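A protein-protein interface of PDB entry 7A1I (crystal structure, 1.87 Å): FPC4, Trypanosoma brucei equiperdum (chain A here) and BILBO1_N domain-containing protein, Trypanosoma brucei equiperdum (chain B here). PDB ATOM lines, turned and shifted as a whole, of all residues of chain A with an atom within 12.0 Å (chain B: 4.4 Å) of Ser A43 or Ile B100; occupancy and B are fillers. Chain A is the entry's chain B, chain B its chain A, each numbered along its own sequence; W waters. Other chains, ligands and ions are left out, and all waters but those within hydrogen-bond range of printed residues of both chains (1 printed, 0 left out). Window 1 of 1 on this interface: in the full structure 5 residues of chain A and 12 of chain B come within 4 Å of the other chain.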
ATOM      1  N   VAL A  40      29.378  -7.786  -5.930  1.00  0.00           N
ATOM      2  CA  VAL A  40      28.547  -7.915  -4.737  1.00  0.00           C
ATOM      3  C   VAL A  40      27.061  -7.884  -5.097  1.00  0.00           C
ATOM      4  O   VAL A  40      26.344  -8.858  -4.874  1.00  0.00           O
ATOM      5  CB  VAL A  40      28.896  -6.824  -3.708  1.00  0.00           C
ATOM      6  CG1 VAL A  40      28.021  -6.949  -2.467  1.00  0.00           C
ATOM      7  CG2 VAL A  40      30.357  -6.929  -3.327  1.00  0.00           C
ATOM      8  N   LEU A  41      26.592  -6.772  -5.661  1.00  0.00           N
ATOM      9  CA  LEU A  41      25.206  -6.663  -6.090  1.00  0.00           C
ATOM     10  C   LEU A  41      25.072  -7.040  -7.556  1.00  0.00           C
ATOM     11  O   LEU A  41      25.845  -6.578  -8.399  1.00  0.00           O
ATOM     12  CB  LEU A  41      24.689  -5.241  -5.888  1.00  0.00           C
ATOM     13  CG  LEU A  41      24.341  -4.854  -4.460  1.00  0.00           C
ATOM     14  CD1 LEU A  41      23.846  -3.417  -4.448  1.00  0.00           C
ATOM     15  CD2 LEU A  41      23.309  -5.809  -3.912  1.00  0.00           C
ATOM     16  N   THR A  42      24.088  -7.875  -7.857  1.00  0.00           N
ATOM     17  CA  THR A  42      23.716  -8.139  -9.237  1.00  0.00           C
ATOM     18  C   THR A  42      22.600  -7.184  -9.634  1.00  0.00           C
ATOM     19  O   THR A  42      21.732  -6.860  -8.821  1.00  0.00           O
ATOM     20  CB  THR A  42      23.277  -9.590  -9.431  1.00  0.00           C
ATOM     21  OG1 THR A  42      22.764  -9.755 -10.759  1.00  0.00           O
ATOM     22  CG2 THR A  42      22.198  -9.955  -8.439  1.00  0.00           C
ATOM     23  N   SER A  43      22.632  -6.730 -10.887  1.00  0.00           N
ATOM     24  CA  SER A  43      21.666  -5.742 -11.346  1.00  0.00           C
ATOM     25  C   SER A  43      20.258  -6.344 -11.413  1.00  0.00           C
ATOM     26  O   SER A  43      20.091  -7.542 -11.663  1.00  0.00           O
ATOM     27  CB  SER A  43      22.076  -5.198 -12.715  1.00  0.00           C
ATOM     28  OG  SER A  43      21.902  -6.142 -13.731  1.00  0.00           O
ATOM     29  N   PRO A  44      19.226  -5.533 -11.195  1.00  0.00           N
ATOM     30  CA  PRO A  44      17.868  -6.070 -11.141  1.00  0.00           C
ATOM     31  C   PRO A  44      17.285  -6.241 -12.534  1.00  0.00           C
ATOM     32  O   PRO A  44      17.741  -5.653 -13.514  1.00  0.00           O
ATOM     33  CB  PRO A  44      17.105  -4.998 -10.357  1.00  0.00           C
ATOM     34  CG  PRO A  44      17.801  -3.720 -10.758  1.00  0.00           C
ATOM     35  CD  PRO A  44      19.255  -4.081 -10.926  1.00  0.00           C
ATOM     36  N   VAL A  45      16.227  -7.038 -12.598  1.00  0.00           N
ATOM     37  CA  VAL A  45      15.468  -7.207 -13.833  1.00  0.00           C
ATOM     38  C   VAL A  45      14.158  -6.446 -13.665  1.00  0.00           C
ATOM     39  O   VAL A  45      13.645  -6.367 -12.543  1.00  0.00           O
ATOM     40  CB  VAL A  45      15.261  -8.702 -14.140  1.00  0.00           C
ATOM     41  CG1 VAL A  45      14.710  -9.430 -12.922  1.00  0.00           C
ATOM     42  CG2 VAL A  45      14.345  -8.900 -15.330  1.00  0.00           C
ATOM     43  N   PRO A  46      13.610  -5.812 -14.720  1.00  0.00           N
ATOM     44  CA  PRO A  46      12.290  -5.180 -14.572  1.00  0.00           C
ATOM     45  C   PRO A  46      11.159  -6.211 -14.518  1.00  0.00           C
ATOM     46  O   PRO A  46      10.288  -6.147 -13.641  1.00  0.00           O
ATOM     47  CB  PRO A  46      12.158  -4.314 -15.833  1.00  0.00           C
ATOM     48  CG  PRO A  46      13.546  -4.247 -16.426  1.00  0.00           C
ATOM     49  CD  PRO A  46      14.228  -5.512 -16.023  1.00  0.00           C
ATOM     50  N   ALA B  11      24.000   3.093 -11.030  1.00  0.00           N
ATOM     51  CA  ALA B  11      24.517   2.192 -12.066  1.00  0.00           C
ATOM     52  C   ALA B  11      23.483   2.068 -13.178  1.00  0.00           C
ATOM     53  O   ALA B  11      22.312   2.434 -13.007  1.00  0.00           O
ATOM     54  CB  ALA B  11      24.877   0.810 -11.496  1.00  0.00           C
ATOM     55  N   LYS B  18      27.672  -3.447 -16.981  1.00  0.00           N
ATOM     56  CA  LYS B  18      27.147  -2.509 -15.987  1.00  0.00           C
ATOM     57  C   LYS B  18      28.195  -1.450 -15.653  1.00  0.00           C
ATOM     58  O   LYS B  18      29.371  -1.776 -15.459  1.00  0.00           O
ATOM     59  CB  LYS B  18      26.689  -3.228 -14.717  1.00  0.00           C
ATOM     60  CG  LYS B  18      25.781  -4.421 -14.987  1.00  0.00           C
ATOM     61  CD  LYS B  18      24.537  -4.028 -15.769  1.00  0.00           C
ATOM     62  CE  LYS B  18      23.780  -5.276 -16.227  1.00  0.00           C
ATOM     63  NZ  LYS B  18      22.509  -4.963 -16.949  1.00  0.00           N
ATOM     64  N   ASN B  20      28.972   1.852 -13.067  1.00  0.00           N
ATOM     65  CA  ASN B  20      28.601   2.367 -11.757  1.00  0.00           C
ATOM     66  C   ASN B  20      29.377   3.656 -11.493  1.00  0.00           C
ATOM     67  O   ASN B  20      30.591   3.695 -11.706  1.00  0.00           O
ATOM     68  CB  ASN B  20      28.906   1.311 -10.683  1.00  0.00           C
ATOM     69  CG  ASN B  20      28.161   1.553  -9.387  1.00  0.00           C
ATOM     70  OD1 ASN B  20      27.216   2.314  -9.343  1.00  0.00           O
ATOM     71  ND2 ASN B  20      28.593   0.890  -8.325  1.00  0.00           N
ATOM     72  N   TRP B  71      15.235  -4.814  -4.499  1.00  0.00           N
ATOM     73  CA  TRP B  71      15.254  -3.555  -5.226  1.00  0.00           C
ATOM     74  C   TRP B  71      13.875  -2.915  -5.128  1.00  0.00           C
ATOM     75  O   TRP B  71      12.878  -3.527  -5.527  1.00  0.00           O
ATOM     76  CB  TRP B  71      15.652  -3.758  -6.684  1.00  0.00           C
ATOM     77  CG  TRP B  71      17.069  -4.208  -6.882  1.00  0.00           C
ATOM     78  CD1 TRP B  71      17.525  -5.505  -6.969  1.00  0.00           C
ATOM     79  CD2 TRP B  71      18.221  -3.369  -7.002  1.00  0.00           C
ATOM     80  NE1 TRP B  71      18.882  -5.512  -7.157  1.00  0.00           N
ATOM     81  CE2 TRP B  71      19.339  -4.219  -7.179  1.00  0.00           C
ATOM     82  CE3 TRP B  71      18.418  -1.981  -6.989  1.00  0.00           C
ATOM     83  CZ2 TRP B  71      20.639  -3.725  -7.333  1.00  0.00           C
ATOM     84  CZ3 TRP B  71      19.707  -1.489  -7.136  1.00  0.00           C
ATOM     85  CH2 TRP B  71      20.807  -2.364  -7.317  1.00  0.00           C
ATOM     86  N   GLN B  85      22.720   2.288  -3.331  1.00  0.00           N
ATOM     87  CA  GLN B  85      23.001   1.888  -4.706  1.00  0.00           C
ATOM     88  C   GLN B  85      21.713   2.044  -5.502  1.00  0.00           C
ATOM     89  O   GLN B  85      20.699   1.398  -5.198  1.00  0.00           O
ATOM     90  CB  GLN B  85      23.518   0.445  -4.801  1.00  0.00           C
ATOM     91  CG  GLN B  85      23.777   0.004  -6.235  1.00  0.00           C
ATOM     92  CD  GLN B  85      25.027   0.674  -6.849  1.00  0.00           C
ATOM     93  OE1 GLN B  85      26.135   0.536  -6.330  1.00  0.00           O
ATOM     94  NE2 GLN B  85      24.833   1.418  -7.928  1.00  0.00           N
ATOM     95  N   TYR B  87      19.875   1.935  -9.386  1.00  0.00           N
ATOM     96  CA  TYR B  87      19.972   1.383 -10.732  1.00  0.00           C
ATOM     97  C   TYR B  87      18.947   2.068 -11.619  1.00  0.00           C
ATOM     98  O   TYR B  87      17.766   2.151 -11.260  1.00  0.00           O
ATOM     99  CB  TYR B  87      19.745  -0.142 -10.759  1.00  0.00           C
ATOM    100  CG  TYR B  87      20.120  -0.765 -12.084  1.00  0.00           C
ATOM    101  CD1 TYR B  87      19.151  -1.066 -13.046  1.00  0.00           C
ATOM    102  CD2 TYR B  87      21.449  -1.072 -12.371  1.00  0.00           C
ATOM    103  CE1 TYR B  87      19.512  -1.649 -14.268  1.00  0.00           C
ATOM    104  CE2 TYR B  87      21.816  -1.642 -13.589  1.00  0.00           C
ATOM    105  CZ  TYR B  87      20.855  -1.919 -14.529  1.00  0.00           C
ATOM    106  OH  TYR B  87      21.227  -2.505 -15.723  1.00  0.00           O
ATOM    107  N   ILE B  96      20.028  -7.277 -19.045  1.00  0.00           N
ATOM    108  CA  ILE B  96      20.241  -8.606 -18.493  1.00  0.00           C
ATOM    109  C   ILE B  96      20.974  -8.445 -17.166  1.00  0.00           C
ATOM    110  O   ILE B  96      21.919  -7.654 -17.077  1.00  0.00           O
ATOM    111  CB  ILE B  96      21.004  -9.501 -19.480  1.00  0.00           C
ATOM    112  CG1 ILE B  96      20.163  -9.706 -20.740  1.00  0.00           C
ATOM    113  CG2 ILE B  96      21.334 -10.881 -18.870  1.00  0.00           C
ATOM    114  CD1 ILE B  96      20.876 -10.480 -21.825  1.00  0.00           C
ATOM    115  N   PRO B  97      20.570  -9.160 -16.119  1.00  0.00           N
ATOM    116  CA  PRO B  97      21.247  -9.024 -14.824  1.00  0.00           C
ATOM    117  C   PRO B  97      22.716  -9.416 -14.901  1.00  0.00           C
ATOM    118  O   PRO B  97      23.083 -10.427 -15.500  1.00  0.00           O
ATOM    119  CB  PRO B  97      20.456  -9.972 -13.914  1.00  0.00           C
ATOM    120  CG  PRO B  97      19.098 -10.037 -14.549  1.00  0.00           C
ATOM    121  CD  PRO B  97      19.359  -9.994 -16.025  1.00  0.00           C
ATOM    122  N   ALA B  98      23.557  -8.592 -14.281  1.00  0.00           N
ATOM    123  CA  ALA B  98      24.986  -8.860 -14.169  1.00  0.00           C
ATOM    124  C   ALA B  98      25.507  -8.123 -12.943  1.00  0.00           C
ATOM    125  O   ALA B  98      24.815  -7.286 -12.358  1.00  0.00           O
ATOM    126  CB  ALA B  98      25.744  -8.419 -15.424  1.00  0.00           C
ATOM    127  N   ALA B  99      26.740  -8.444 -12.565  1.00  0.00           N
ATOM    128  CA  ALA B  99      27.339  -7.843 -11.381  1.00  0.00           C
ATOM    129  C   ALA B  99      27.541  -6.347 -11.586  1.00  0.00           C
ATOM    130  O   ALA B  99      27.990  -5.902 -12.646  1.00  0.00           O
ATOM    131  CB  ALA B  99      28.674  -8.520 -11.065  1.00  0.00           C
ATOM    132  N   ILE B 100      27.195  -5.560 -10.573  1.00  0.00           N
ATOM    133  CA  ILE B 100      27.445  -4.125 -10.589  1.00  0.00           C
ATOM    134  C   ILE B 100      28.858  -3.896 -10.064  1.00  0.00           C
ATOM    135  O   ILE B 100      29.173  -4.347  -8.951  1.00  0.00           O
ATOM    136  CB  ILE B 100      26.410  -3.356  -9.762  1.00  0.00           C
ATOM    137  CG1 ILE B 100      25.017  -3.526 -10.387  1.00  0.00           C
ATOM    138  CG2 ILE B 100      26.783  -1.907  -9.731  1.00  0.00           C
ATOM    139  CD1 ILE B 100      23.873  -3.010  -9.494  1.00  0.00           C
ATOM    140  N   PRO B 101      29.725  -3.233 -10.810  1.00  0.00           N
ATOM    141  CA  PRO B 101      31.119  -3.089 -10.385  1.00  0.00           C
ATOM    142  C   PRO B 101      31.314  -1.961  -9.377  1.00  0.00           C
ATOM    143  O   PRO B 101      30.405  -1.196  -9.058  1.00  0.00           O
ATOM    144  CB  PRO B 101      31.848  -2.773 -11.687  1.00  0.00           C
ATOM    145  CG  PRO B 101      30.833  -2.126 -12.536  1.00  0.00           C
ATOM    146  CD  PRO B 101      29.502  -2.716 -12.171  1.00  0.00           C
ATOM    147  N   GLU B 102      32.547  -1.882  -8.881  1.00  0.00           N
ATOM    148  CA  GLU B 102      32.976  -0.731  -8.107  1.00  0.00           C
ATOM    149  C   GLU B 102      32.731   0.533  -8.930  1.00  0.00           C
ATOM    150  O   GLU B 102      32.829   0.510 -10.162  1.00  0.00           O
ATOM    151  CB  GLU B 102      34.466  -0.820  -7.790  1.00  0.00           C
ATOM    152  CG  GLU B 102      34.948  -2.127  -7.192  1.00  0.00           C
ATOM    153  CD  GLU B 102      34.536  -2.323  -5.756  1.00  0.00           C
ATOM    154  OE1 GLU B 102      34.530  -3.490  -5.304  1.00  0.00           O
ATOM    155  OE2 GLU B 102      34.248  -1.318  -5.074  1.00  0.00           O
HETATM  156  O   HOH W   1      19.878  -5.689 -15.072  1.00  0.00           O
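Water W1 lies within hydrogen-bond range of the side-chain hydroxyl (OG) of Ser A43 (2.5 Å), the backbone carbonyl oxygen (O) of Pro A44 (2.6 Å), the side-chain amino group (NZ) of Lys B18 (3.3 Å) and the backbone carbonyl oxygen (O) of Ile B96 (3.5 Å).
O of Leu A41 touches CA of Ala B99 (3.6 Å). Thr A42 touches Trp B71 (O to NE1, 3.6 Å). OG1 of Thr A42 touches CB of Pro B97 (3.9 Å). Ala B98 touches Thr A42 (O to CA, 3.4 Å). Ser A43 touches Tyr B87 (CB to CE2, 3.7 Å). O of Ile B96 touches OG of Ser A43, 3.7 Å away. Pro B97 touches Ser A43. Ile B100 touches Ser A43. Pro A44 touches Trp B71 (CB to CD1, 3.5 Å). Pro A44 touches Tyr B87.
The backbone carbonyl oxygen of Leu A41 sits at hydrogen-bond distance from the backbone NH of Ile B100 (2.8 Å). The backbone carbonyl oxygen (O) of Ala B98 is in hydrogen-bond range of the backbone NH (N) of Ser A43 (2.7 Å). OG of Ser A43 sits close to NZ of Lys B18, 3.5 Å away.
Hydrophobic or aromatic side chains of chain B within 4 Å of the printed part of chain A: Trp B71, Tyr B87, Pro B97 and Ile B100. Along chain B the printed residues that touch a printed residue of chain A span positions 18 to 100. Of the 7 printed residues of chain A, 4 touch a printed residue of chain B. Printed residues of chain A that touch a printed residue of chain B: Leu A41, Thr A42, Ser A43 and Pro A44. Hydrophobic or aromatic side chains of chain A that line the printed part of chain B: Leu A41 and Pro A44. Among the printed residues, 14 pairs touch across the chains. Among the printed residues, no Asp or Glu carboxylate lies within 4 Å of a Lys or Arg side-chain nitrogen of the other chain.
OH of Tyr B87 lies within hydrogen-bond range of NZ of Lys B18, 3.0 Å away. The side-chain amide nitrogen (NE2) of Gln B85 sits at hydrogen-bond distance from the side-chain amide oxygen (OD1) of Asn B20 (2.9 Å). The side-chain amino group of Lys B18 sits at hydrogen-bond distance from the backbone carbonyl oxygen of Ile B96.
Printed residues of chain B within 4 Å of Ser A43: Lys B18, Tyr B87, Ile B96, Pro B97, Ala B98 and Ile B100. Ile B100 touches two residues of chain A. Ala B11 touches none of the printed residues of chain A. Asn B20 touches none of the printed residues of chain A. Pro B97 touches just these residues of chain A: Thr A42 and Ser A43. Ala B98 touches two residues of chain A. Ala B99 touches one residue of chain A. No residue of chain A comes within 4 Å of Pro B101. No residue of chain A comes within 4 Å of Glu B102. Printed residues of chain B within 4 Å of Thr A42: Trp B71, Pro B97 and Ala B98. Printed residues of chain A within 4 Å of Gln B85: Leu A41. Printed residues of chain B within 4 Å of Leu A41: Gln B85, Ala B99 and Ile B100. The nearest printed residue of chain A that does not touch Trp B71 is Leu A41 (4.3 Å).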
